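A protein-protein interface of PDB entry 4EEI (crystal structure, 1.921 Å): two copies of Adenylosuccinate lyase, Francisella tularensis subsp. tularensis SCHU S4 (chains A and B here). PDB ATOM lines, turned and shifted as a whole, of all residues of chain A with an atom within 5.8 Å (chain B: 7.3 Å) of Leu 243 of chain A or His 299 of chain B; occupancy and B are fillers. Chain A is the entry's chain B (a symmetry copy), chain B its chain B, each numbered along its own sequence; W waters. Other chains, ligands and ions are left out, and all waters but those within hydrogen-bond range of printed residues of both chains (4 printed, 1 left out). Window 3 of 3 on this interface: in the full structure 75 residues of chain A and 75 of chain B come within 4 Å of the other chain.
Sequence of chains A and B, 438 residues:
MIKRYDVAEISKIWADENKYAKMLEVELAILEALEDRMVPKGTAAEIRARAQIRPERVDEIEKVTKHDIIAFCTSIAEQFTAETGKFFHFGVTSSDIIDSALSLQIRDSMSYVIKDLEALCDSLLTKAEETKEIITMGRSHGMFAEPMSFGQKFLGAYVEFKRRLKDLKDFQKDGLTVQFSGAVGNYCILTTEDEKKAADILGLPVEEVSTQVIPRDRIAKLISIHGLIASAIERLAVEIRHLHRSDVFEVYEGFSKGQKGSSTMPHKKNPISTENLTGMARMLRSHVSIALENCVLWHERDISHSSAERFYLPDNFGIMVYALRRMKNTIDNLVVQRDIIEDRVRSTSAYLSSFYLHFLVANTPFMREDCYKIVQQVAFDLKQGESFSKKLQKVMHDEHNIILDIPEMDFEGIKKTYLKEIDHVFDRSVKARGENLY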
ATOM      1  N   ARG A 139      -5.019 -28.838  -6.669  1.00  0.00           N
ATOM      2  CA  ARG A 139      -4.986 -28.888  -8.123  1.00  0.00           C
ATOM      3  C   ARG A 139      -3.637 -29.375  -8.623  1.00  0.00           C
ATOM      4  O   ARG A 139      -2.584 -28.873  -8.211  1.00  0.00           O
ATOM      5  CB  ARG A 139      -5.249 -27.494  -8.716  1.00  0.00           C
ATOM      6  CG  ARG A 139      -6.704 -26.986  -8.603  1.00  0.00           C
ATOM      7  CD  ARG A 139      -6.795 -25.567  -9.172  1.00  0.00           C
ATOM      8  NE  ARG A 139      -8.070 -24.887  -8.898  1.00  0.00           N
ATOM      9  CZ  ARG A 139      -8.346 -24.243  -7.763  1.00  0.00           C
ATOM     10  NH1 ARG A 139      -7.458 -24.213  -6.774  1.00  0.00           N
ATOM     11  NH2 ARG A 139      -9.514 -23.634  -7.610  1.00  0.00           N
ATOM     12  N   SER A 140      -3.659 -30.367  -9.506  1.00  0.00           N
ATOM     13  CA  SER A 140      -2.440 -30.823 -10.163  1.00  0.00           C
ATOM     14  C   SER A 140      -2.643 -30.707 -11.664  1.00  0.00           C
ATOM     15  O   SER A 140      -3.685 -31.105 -12.187  1.00  0.00           O
ATOM     16  CB  SER A 140      -2.116 -32.259  -9.772  1.00  0.00           C
ATOM     17  OG  SER A 140      -3.223 -33.099 -10.008  1.00  0.00           O
ATOM     18  N   GLY A 142      -3.214 -27.966 -12.840  1.00  0.00           N
ATOM     19  CA  GLY A 142      -4.324 -27.016 -12.851  1.00  0.00           C
ATOM     20  C   GLY A 142      -5.700 -27.661 -12.776  1.00  0.00           C
ATOM     21  O   GLY A 142      -6.723 -26.962 -12.782  1.00  0.00           O
ATOM     22  N   PHE A 150      -6.593 -24.998   2.906  1.00  0.00           N
ATOM     23  CA  PHE A 150      -6.153 -23.805   2.176  1.00  0.00           C
ATOM     24  C   PHE A 150      -4.907 -23.244   2.851  1.00  0.00           C
ATOM     25  O   PHE A 150      -3.982 -22.757   2.187  1.00  0.00           O
ATOM     26  CB  PHE A 150      -7.273 -22.759   2.166  1.00  0.00           C
ATOM     27  CG  PHE A 150      -7.038 -21.603   1.216  1.00  0.00           C
ATOM     28  CD1 PHE A 150      -6.507 -20.408   1.672  1.00  0.00           C
ATOM     29  CD2 PHE A 150      -7.371 -21.711  -0.130  1.00  0.00           C
ATOM     30  CE1 PHE A 150      -6.314 -19.334   0.802  1.00  0.00           C
ATOM     31  CE2 PHE A 150      -7.170 -20.647  -1.006  1.00  0.00           C
ATOM     32  CZ  PHE A 150      -6.646 -19.458  -0.535  1.00  0.00           C
ATOM     33  N   LYS A 153      -1.327 -23.994   1.756  1.00  0.00           N
ATOM     34  CA  LYS A 153      -0.696 -23.240   0.667  1.00  0.00           C
ATOM     35  C   LYS A 153       0.275 -22.228   1.261  1.00  0.00           C
ATOM     36  O   LYS A 153       1.428 -22.128   0.843  1.00  0.00           O
ATOM     37  CB  LYS A 153      -1.737 -22.522  -0.197  1.00  0.00           C
ATOM     38  CG  LYS A 153      -2.646 -23.452  -1.008  1.00  0.00           C
ATOM     39  CD  LYS A 153      -3.751 -22.649  -1.696  1.00  0.00           C
ATOM     40  CE  LYS A 153      -4.585 -23.517  -2.647  1.00  0.00           C
ATOM     41  NZ  LYS A 153      -3.764 -24.091  -3.755  1.00  0.00           N
ATOM     42  N   ARG A 235       7.265 -18.288  -6.824  1.00  0.00           N
ATOM     43  CA  ARG A 235       6.316 -19.383  -6.652  1.00  0.00           C
ATOM     44  C   ARG A 235       5.101 -18.902  -5.893  1.00  0.00           C
ATOM     45  O   ARG A 235       3.979 -19.238  -6.255  1.00  0.00           O
ATOM     46  CB  ARG A 235       6.949 -20.581  -5.938  1.00  0.00           C
ATOM     47  CG  ARG A 235       6.038 -21.818  -5.899  1.00  0.00           C
ATOM     48  CD  ARG A 235       6.792 -23.062  -5.427  1.00  0.00           C
ATOM     49  NE  ARG A 235       7.063 -23.030  -3.995  1.00  0.00           N
ATOM     50  CZ  ARG A 235       6.258 -23.563  -3.080  1.00  0.00           C
ATOM     51  NH1 ARG A 235       6.568 -23.495  -1.787  1.00  0.00           N
ATOM     52  NH2 ARG A 235       5.135 -24.165  -3.454  1.00  0.00           N
ATOM     53  N   VAL A 238       2.996 -16.393  -8.039  1.00  0.00           N
ATOM     54  CA  VAL A 238       2.231 -17.077  -9.076  1.00  0.00           C
ATOM     55  C   VAL A 238       1.010 -17.769  -8.474  1.00  0.00           C
ATOM     56  O   VAL A 238      -0.082 -17.766  -9.057  1.00  0.00           O
ATOM     57  CB  VAL A 238       3.130 -18.087  -9.809  1.00  0.00           C
ATOM     58  CG1 VAL A 238       2.304 -19.049 -10.670  1.00  0.00           C
ATOM     59  CG2 VAL A 238       4.173 -17.347 -10.656  1.00  0.00           C
ATOM     60  N   GLU A 239       1.184 -18.355  -7.295  1.00  0.00           N
ATOM     61  CA  GLU A 239       0.053 -18.949  -6.591  1.00  0.00           C
ATOM     62  C   GLU A 239      -1.038 -17.909  -6.345  1.00  0.00           C
ATOM     63  O   GLU A 239      -2.221 -18.155  -6.599  1.00  0.00           O
ATOM     64  CB  GLU A 239       0.510 -19.561  -5.264  1.00  0.00           C
ATOM     65  CG  GLU A 239      -0.625 -20.140  -4.420  1.00  0.00           C
ATOM     66  CD  GLU A 239      -1.189 -21.450  -4.961  1.00  0.00           C
ATOM     67  OE1 GLU A 239      -0.476 -22.149  -5.709  1.00  0.00           O
ATOM     68  OE2 GLU A 239      -2.350 -21.787  -4.621  1.00  0.00           O
ATOM     69  N   ILE A 240      -0.658 -16.739  -5.856  1.00  0.00           N
ATOM     70  CA  ILE A 240      -1.670 -15.717  -5.610  1.00  0.00           C
ATOM     71  C   ILE A 240      -2.316 -15.252  -6.925  1.00  0.00           C
ATOM     72  O   ILE A 240      -3.539 -15.066  -6.988  1.00  0.00           O
ATOM     73  CB  ILE A 240      -1.099 -14.548  -4.795  1.00  0.00           C
ATOM     74  CG1 ILE A 240      -0.779 -15.029  -3.378  1.00  0.00           C
ATOM     75  CG2 ILE A 240      -2.102 -13.395  -4.710  1.00  0.00           C
ATOM     76  CD1 ILE A 240       0.167 -14.118  -2.615  1.00  0.00           C
ATOM     77  N   ARG A 241      -1.510 -15.093  -7.973  1.00  0.00           N
ATOM     78  CA  ARG A 241      -2.031 -14.642  -9.269  1.00  0.00           C
ATOM     79  C   ARG A 241      -3.046 -15.621  -9.848  1.00  0.00           C
ATOM     80  O   ARG A 241      -4.050 -15.211 -10.439  1.00  0.00           O
ATOM     81  CB  ARG A 241      -0.886 -14.409 -10.262  1.00  0.00           C
ATOM     82  CG  ARG A 241      -0.034 -13.168  -9.968  1.00  0.00           C
ATOM     83  CD  ARG A 241       1.277 -13.204 -10.758  1.00  0.00           C
ATOM     84  NE  ARG A 241       1.049 -13.287 -12.198  1.00  0.00           N
ATOM     85  CZ  ARG A 241       1.998 -13.558 -13.087  1.00  0.00           C
ATOM     86  NH1 ARG A 241       3.243 -13.773 -12.684  1.00  0.00           N
ATOM     87  NH2 ARG A 241       1.699 -13.628 -14.375  1.00  0.00           N
ATOM     88  N   HIS A 242      -2.776 -16.911  -9.683  1.00  0.00           N
ATOM     89  CA  HIS A 242      -3.710 -17.967 -10.091  1.00  0.00           C
ATOM     90  C   HIS A 242      -5.029 -17.876  -9.330  1.00  0.00           C
ATOM     91  O   HIS A 242      -6.105 -17.950  -9.917  1.00  0.00           O
ATOM     92  CB  HIS A 242      -3.113 -19.348  -9.800  1.00  0.00           C
ATOM     93  CG  HIS A 242      -2.158 -19.836 -10.834  1.00  0.00           C
ATOM     94  ND1 HIS A 242      -2.443 -19.820 -12.183  1.00  0.00           N
ATOM     95  CD2 HIS A 242      -0.932 -20.413 -10.715  1.00  0.00           C
ATOM     96  CE1 HIS A 242      -1.429 -20.349 -12.852  1.00  0.00           C
ATOM     97  NE2 HIS A 242      -0.500 -20.705 -11.979  1.00  0.00           N
ATOM     98  N   LEU A 243      -4.937 -17.744  -8.012  1.00  0.00           N
ATOM     99  CA  LEU A 243      -6.121 -17.727  -7.168  1.00  0.00           C
ATOM    100  C   LEU A 243      -6.924 -16.435  -7.352  1.00  0.00           C
ATOM    101  O   LEU A 243      -8.113 -16.387  -7.047  1.00  0.00           O
ATOM    102  CB  LEU A 243      -5.728 -17.912  -5.695  1.00  0.00           C
ATOM    103  CG  LEU A 243      -5.033 -19.220  -5.308  1.00  0.00           C
ATOM    104  CD1 LEU A 243      -4.555 -19.124  -3.873  1.00  0.00           C
ATOM    105  CD2 LEU A 243      -5.960 -20.419  -5.467  1.00  0.00           C
ATOM    106  N   HIS A 244      -6.268 -15.398  -7.869  1.00  0.00           N
ATOM    107  CA  HIS A 244      -6.874 -14.077  -8.021  1.00  0.00           C
ATOM    108  C   HIS A 244      -7.647 -13.965  -9.348  1.00  0.00           C
ATOM    109  O   HIS A 244      -8.500 -13.101  -9.498  1.00  0.00           O
ATOM    110  CB  HIS A 244      -5.763 -13.018  -7.949  1.00  0.00           C
ATOM    111  CG  HIS A 244      -6.239 -11.630  -7.652  1.00  0.00           C
ATOM    112  ND1 HIS A 244      -7.350 -11.070  -8.243  1.00  0.00           N
ATOM    113  CD2 HIS A 244      -5.724 -10.674  -6.840  1.00  0.00           C
ATOM    114  CE1 HIS A 244      -7.510  -9.834  -7.797  1.00  0.00           C
ATOM    115  NE2 HIS A 244      -6.527  -9.568  -6.951  1.00  0.00           N
ATOM    116  N   ARG A 245      -7.363 -14.844 -10.309  1.00  0.00           N
ATOM    117  CA  ARG A 245      -7.973 -14.706 -11.639  1.00  0.00           C
ATOM    118  C   ARG A 245      -9.502 -14.806 -11.592  1.00  0.00           C
ATOM    119  O   ARG A 245     -10.055 -15.464 -10.707  1.00  0.00           O
ATOM    120  CB  ARG A 245      -7.366 -15.705 -12.644  1.00  0.00           C
ATOM    121  CG  ARG A 245      -7.698 -17.166 -12.387  1.00  0.00           C
ATOM    122  CD  ARG A 245      -7.108 -18.085 -13.465  1.00  0.00           C
ATOM    123  NE  ARG A 245      -7.744 -17.846 -14.759  1.00  0.00           N
ATOM    124  CZ  ARG A 245      -7.112 -17.865 -15.932  1.00  0.00           C
ATOM    125  NH1 ARG A 245      -5.811 -18.126 -16.002  1.00  0.00           N
ATOM    126  NH2 ARG A 245      -7.789 -17.614 -17.043  1.00  0.00           N
ATOM    127  N   VAL A 248     -11.173 -18.232 -11.039  1.00  0.00           N
ATOM    128  CA  VAL A 248     -11.085 -18.845  -9.718  1.00  0.00           C
ATOM    129  C   VAL A 248     -11.578 -17.920  -8.608  1.00  0.00           C
ATOM    130  O   VAL A 248     -12.438 -18.296  -7.814  1.00  0.00           O
ATOM    131  CB  VAL A 248      -9.633 -19.247  -9.402  1.00  0.00           C
ATOM    132  CG1 VAL A 248      -9.578 -20.119  -8.159  1.00  0.00           C
ATOM    133  CG2 VAL A 248      -9.008 -19.956 -10.594  1.00  0.00           C
ATOM    134  N   PHE A 249     -11.038 -16.708  -8.569  1.00  0.00           N
ATOM    135  CA  PHE A 249     -11.507 -15.668  -7.655  1.00  0.00           C
ATOM    136  C   PHE A 249     -11.580 -16.094  -6.186  1.00  0.00           C
ATOM    137  O   PHE A 249     -12.549 -15.774  -5.501  1.00  0.00           O
ATOM    138  CB  PHE A 249     -12.849 -15.092  -8.109  1.00  0.00           C
ATOM    139  CG  PHE A 249     -13.047 -13.655  -7.719  1.00  0.00           C
ATOM    140  CD1 PHE A 249     -11.994 -12.759  -7.783  1.00  0.00           C
ATOM    141  CD2 PHE A 249     -14.278 -13.203  -7.281  1.00  0.00           C
ATOM    142  CE1 PHE A 249     -12.166 -11.437  -7.422  1.00  0.00           C
ATOM    143  CE2 PHE A 249     -14.459 -11.882  -6.918  1.00  0.00           C
ATOM    144  CZ  PHE A 249     -13.401 -10.998  -6.989  1.00  0.00           C
ATOM    145  N   GLU A 250     -10.572 -16.811  -5.700  1.00  0.00           N
ATOM    146  CA  GLU A 250     -10.587 -17.270  -4.314  1.00  0.00           C
ATOM    147  C   GLU A 250      -9.935 -16.256  -3.367  1.00  0.00           C
ATOM    148  O   GLU A 250     -10.186 -16.279  -2.160  1.00  0.00           O
ATOM    149  CB  GLU A 250      -9.937 -18.660  -4.214  1.00  0.00           C
ATOM    150  CG  GLU A 250     -10.802 -19.760  -4.856  1.00  0.00           C
ATOM    151  CD  GLU A 250     -10.194 -21.160  -4.802  1.00  0.00           C
ATOM    152  OE1 GLU A 250      -9.083 -21.329  -4.237  1.00  0.00           O
ATOM    153  OE2 GLU A 250     -10.842 -22.096  -5.335  1.00  0.00           O
ATOM    154  N   VAL A 251      -9.107 -15.365  -3.913  1.00  0.00           N
ATOM    155  CA  VAL A 251      -8.529 -14.269  -3.126  1.00  0.00           C
ATOM    156  C   VAL A 251      -8.505 -12.992  -3.958  1.00  0.00           C
ATOM    157  O   VAL A 251      -8.651 -13.043  -5.177  1.00  0.00           O
ATOM    158  CB  VAL A 251      -7.058 -14.551  -2.715  1.00  0.00           C
ATOM    159  CG1 VAL A 251      -6.924 -15.894  -2.011  1.00  0.00           C
ATOM    160  CG2 VAL A 251      -6.151 -14.520  -3.947  1.00  0.00           C
ATOM    161  N   THR B 211       3.482 -31.302  -1.464  1.00  0.00           N
ATOM    162  CA  THR B 211       2.249 -31.187  -2.225  1.00  0.00           C
ATOM    163  C   THR B 211       1.900 -32.540  -2.832  1.00  0.00           C
ATOM    164  O   THR B 211       2.084 -33.573  -2.193  1.00  0.00           O
ATOM    165  CB  THR B 211       2.351 -30.119  -3.331  1.00  0.00           C
ATOM    166  OG1 THR B 211       3.532 -30.338  -4.111  1.00  0.00           O
ATOM    167  CG2 THR B 211       2.403 -28.728  -2.721  1.00  0.00           C
ATOM    168  N   GLN B 212       1.647 -32.541  -4.133  1.00  0.00           N
ATOM    169  CA  GLN B 212       1.768 -33.770  -4.888  1.00  0.00           C
ATOM    170  C   GLN B 212       3.253 -34.106  -4.925  1.00  0.00           C
ATOM    171  O   GLN B 212       3.641 -35.272  -4.896  1.00  0.00           O
ATOM    172  CB  GLN B 212       1.215 -33.614  -6.303  1.00  0.00           C
ATOM    173  CG  GLN B 212       1.262 -34.897  -7.117  1.00  0.00           C
ATOM    174  CD  GLN B 212       0.243 -34.919  -8.237  1.00  0.00           C
ATOM    175  OE1 GLN B 212       0.579 -34.703  -9.399  1.00  0.00           O
ATOM    176  NE2 GLN B 212      -1.011 -35.184  -7.892  1.00  0.00           N
ATOM    177  N   VAL B 213       4.077 -33.065  -5.014  1.00  0.00           N
ATOM    178  CA  VAL B 213       5.511 -33.218  -5.222  1.00  0.00           C
ATOM    179  C   VAL B 213       6.303 -32.742  -4.009  1.00  0.00           C
ATOM    180  O   VAL B 213       5.773 -32.049  -3.142  1.00  0.00           O
ATOM    181  CB  VAL B 213       5.987 -32.443  -6.462  1.00  0.00           C
ATOM    182  CG1 VAL B 213       5.351 -33.012  -7.720  1.00  0.00           C
ATOM    183  CG2 VAL B 213       5.665 -30.964  -6.317  1.00  0.00           C
ATOM    184  N   VAL B 296       9.162 -22.986  -9.793  1.00  0.00           N
ATOM    185  CA  VAL B 296       7.892 -22.257  -9.902  1.00  0.00           C
ATOM    186  C   VAL B 296       6.790 -23.133 -10.495  1.00  0.00           C
ATOM    187  O   VAL B 296       6.343 -22.918 -11.631  1.00  0.00           O
ATOM    188  CB  VAL B 296       8.074 -20.956 -10.714  1.00  0.00           C
ATOM    189  CG1 VAL B 296       6.848 -20.052 -10.570  1.00  0.00           C
ATOM    190  CG2 VAL B 296       9.325 -20.232 -10.223  1.00  0.00           C
ATOM    191  N   LEU B 297       6.356 -24.123  -9.711  1.00  0.00           N
ATOM    192  CA  LEU B 297       5.284 -25.026 -10.119  1.00  0.00           C
ATOM    193  C   LEU B 297       3.901 -24.488  -9.758  1.00  0.00           C
ATOM    194  O   LEU B 297       3.728 -23.824  -8.730  1.00  0.00           O
ATOM    195  CB  LEU B 297       5.485 -26.394  -9.464  1.00  0.00           C
ATOM    196  CG  LEU B 297       6.840 -27.047  -9.745  1.00  0.00           C
ATOM    197  CD1 LEU B 297       6.919 -28.403  -9.052  1.00  0.00           C
ATOM    198  CD2 LEU B 297       7.107 -27.180 -11.257  1.00  0.00           C
ATOM    199  N   TRP B 298       2.916 -24.783 -10.598  1.00  0.00           N
ATOM    200  CA  TRP B 298       1.564 -24.309 -10.383  1.00  0.00           C
ATOM    201  C   TRP B 298       0.849 -25.095  -9.324  1.00  0.00           C
ATOM    202  O   TRP B 298       0.782 -26.339  -9.385  1.00  0.00           O
ATOM    203  CB  TRP B 298       0.771 -24.366 -11.680  1.00  0.00           C
ATOM    204  CG  TRP B 298       1.203 -23.342 -12.699  1.00  0.00           C
ATOM    205  CD1 TRP B 298       2.328 -22.526 -12.661  1.00  0.00           C
ATOM    206  CD2 TRP B 298       0.520 -22.992 -13.949  1.00  0.00           C
ATOM    207  NE1 TRP B 298       2.384 -21.722 -13.768  1.00  0.00           N
ATOM    208  CE2 TRP B 298       1.332 -21.951 -14.581  1.00  0.00           C
ATOM    209  CE3 TRP B 298      -0.635 -23.420 -14.582  1.00  0.00           C
ATOM    210  CZ2 TRP B 298       0.981 -21.381 -15.788  1.00  0.00           C
ATOM    211  CZ3 TRP B 298      -0.978 -22.837 -15.802  1.00  0.00           C
ATOM    212  CH2 TRP B 298      -0.188 -21.843 -16.387  1.00  0.00           C
ATOM    213  N   HIS B 299       0.356 -24.387  -8.316  1.00  0.00           N
ATOM    214  CA  HIS B 299      -0.466 -24.975  -7.282  1.00  0.00           C
ATOM    215  C   HIS B 299       0.216 -26.146  -6.644  1.00  0.00           C
ATOM    216  O   HIS B 299       1.421 -26.088  -6.330  1.00  0.00           O
ATOM    217  CB  HIS B 299      -1.827 -25.371  -7.839  1.00  0.00           C
ATOM    218  CG  HIS B 299      -2.678 -24.193  -8.247  1.00  0.00           C
ATOM    219  ND1 HIS B 299      -2.915 -23.155  -7.426  1.00  0.00           N
ATOM    220  CD2 HIS B 299      -3.347 -23.913  -9.436  1.00  0.00           C
ATOM    221  CE1 HIS B 299      -3.697 -22.258  -8.052  1.00  0.00           C
ATOM    222  NE2 HIS B 299      -3.961 -22.723  -9.282  1.00  0.00           N
ATOM    223  N   GLU B 300      -0.480 -27.275  -6.562  1.00  0.00           N
ATOM    224  CA  GLU B 300       0.049 -28.447  -5.872  1.00  0.00           C
ATOM    225  C   GLU B 300       0.953 -29.275  -6.779  1.00  0.00           C
ATOM    226  O   GLU B 300       1.366 -30.376  -6.421  1.00  0.00           O
ATOM    227  CB  GLU B 300      -1.084 -29.303  -5.307  1.00  0.00           C
ATOM    228  CG  GLU B 300      -1.743 -28.704  -4.075  1.00  0.00           C
ATOM    229  CD  GLU B 300      -2.432 -27.387  -4.373  1.00  0.00           C
ATOM    230  OE1 GLU B 300      -3.274 -27.355  -5.293  1.00  0.00           O
ATOM    231  OE2 GLU B 300      -2.130 -26.387  -3.692  1.00  0.00           O
ATOM    232  N   ARG B 301       1.260 -28.731  -7.952  1.00  0.00           N
ATOM    233  CA  ARG B 301       2.229 -29.345  -8.852  1.00  0.00           C
ATOM    234  C   ARG B 301       1.854 -29.264 -10.325  1.00  0.00           C
ATOM    235  O   ARG B 301       0.681 -29.230 -10.692  1.00  0.00           O
ATOM    236  CB  ARG B 301       2.504 -30.802  -8.461  1.00  0.00           C
ATOM    237  CG  ARG B 301       1.710 -31.837  -9.246  1.00  0.00           C
ATOM    238  CD  ARG B 301       2.182 -31.956 -10.688  1.00  0.00           C
ATOM    239  NE  ARG B 301       3.572 -32.393 -10.796  1.00  0.00           N
ATOM    240  CZ  ARG B 301       3.985 -33.640 -10.602  1.00  0.00           C
ATOM    241  NH1 ARG B 301       3.116 -34.590 -10.282  1.00  0.00           N
ATOM    242  NH2 ARG B 301       5.270 -33.940 -10.724  1.00  0.00           N
ATOM    243  N   ASP B 302       2.885 -29.235 -11.158  1.00  0.00           N
ATOM    244  CA  ASP B 302       2.744 -29.324 -12.598  1.00  0.00           C
ATOM    245  C   ASP B 302       4.019 -29.960 -13.131  1.00  0.00           C
ATOM    246  O   ASP B 302       5.017 -30.015 -12.418  1.00  0.00           O
ATOM    247  CB  ASP B 302       2.519 -27.944 -13.217  1.00  0.00           C
ATOM    248  CG  ASP B 302       3.814 -27.217 -13.521  1.00  0.00           C
ATOM    249  OD1 ASP B 302       3.991 -26.087 -13.024  1.00  0.00           O
ATOM    250  OD2 ASP B 302       4.653 -27.775 -14.256  1.00  0.00           O
HETATM  251  O   HOH W   1       0.655 -21.817  -8.060  1.00  0.00           O
HETATM  252  O   HOH W   2       3.317 -21.208  -8.065  1.00  0.00           O
HETATM  253  O   HOH W   3       3.452 -24.420  -6.060  1.00  0.00           O
HETATM  254  O   HOH W   4      -5.201 -25.622  -5.577  1.00  0.00           O
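Printed residues of chain B within 4 Å of Leu 243 of chain A: His 299 (3.9 Å). Val 248 of chain A touches none of the printed residues of chain B. Printed residues of chain A within 4 Å of Gln 212 of chain B: Ser 140 (3.6 Å). His 299 of chain B touches just these residues of chain A: Arg 139 (3.6 Å), Lys 153 (3.9 Å), Glu 239 (3.1 Å), His 242 (3.4 Å) and Leu 243 (3.9 Å). Printed residues of chain A within 4 Å of Arg 301 of chain B: Arg 139 and Ser 140.
No position is printed for both chains.
Among the printed residues, merely in contact across the chains: His 242 of chain A with Trp 298 of chain B, His 242 of chain A with His 299 of chain B, Ser 140 of chain A with Arg 301 of chain B, Arg 139 of chain A with His 299 of chain B, Ser 140 of chain A with Gln 212 of chain B, Val 238 of chain A with Val 296 of chain B, Arg 139 of chain A with Arg 301 of chain B, Lys 153 of chain A with His 299 of chain B and Leu 243 of chain A with His 299 of chain B.
OG1 of Thr 211 of chain B lies within hydrogen-bond range of O of Glu 300 of chain B (3.2 Å). The backbone NH (N) of Gln 212 of chain B sits at hydrogen-bond distance from the backbone carbonyl oxygen (O) of Glu 300 of chain B (3.2 Å). The side-chain amide oxygen (OE1) of Gln 212 of chain B sits at hydrogen-bond distance from the guanidinium group (NH1) of Arg 301 of chain B (2.7 Å). O of Leu 243 of chain A sits at hydrogen-bond distance from N of Phe 249 of chain A. The backbone carbonyl oxygen (O) of Leu 243 of chain A lies within hydrogen-bond range of the backbone NH (N) of Glu 250 of chain A. N of Val 251 of chain A sits at hydrogen-bond distance from O of Leu 243 of chain A (3.4 Å).
Hydrophobic or aromatic side chains of chain B that line the printed part of chain A: Val 296, Trp 298 and His 299. Of the 18 printed residues of chain A, 7 touch a printed residue of chain B. Hydrophobic or aromatic side chains of chain A that line the printed part of chain B: Val 238, His 242 and Leu 243. Among the printed residues, 12 pairs touch across the chains.
Water W1 bridges the backbone NH (N) of His 299 of chain B and the side-chain carboxylate (OE1) of Glu 239 of chain A. Water W4 lies within hydrogen-bond range of OE1 of Glu 300 of chain B (2.6 Å), NZ of Lys 153 of chain A (2.8 Å) and NH1 of Arg 139 of chain A (2.9 Å). Water W3 lies within hydrogen-bond range of O of His 299 of chain B (2.6 Å), O of Leu 297 of chain B (2.7 Å) and NH2 of Arg 235 of chain A (3.1 Å). Water W2 lies within hydrogen-bond range of the backbone carbonyl oxygen (O) of Leu 297 of chain B and the backbone carbonyl oxygen (O) of Arg 235 of chain A.
OE1 of Glu 239 of chain A is in hydrogen-bond range of ND1 of His 299 of chain B, 3.1 Å away. The backbone NH of Arg 139 of chain A sits at hydrogen-bond distance from the side-chain carboxylate of Glu 300 of chain B (2.7 Å). The side-chain carboxylate (OE2) of Glu 300 of chain B lies within salt-bridge range of the side-chain amino group (NZ) of Lys 153 of chain A.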
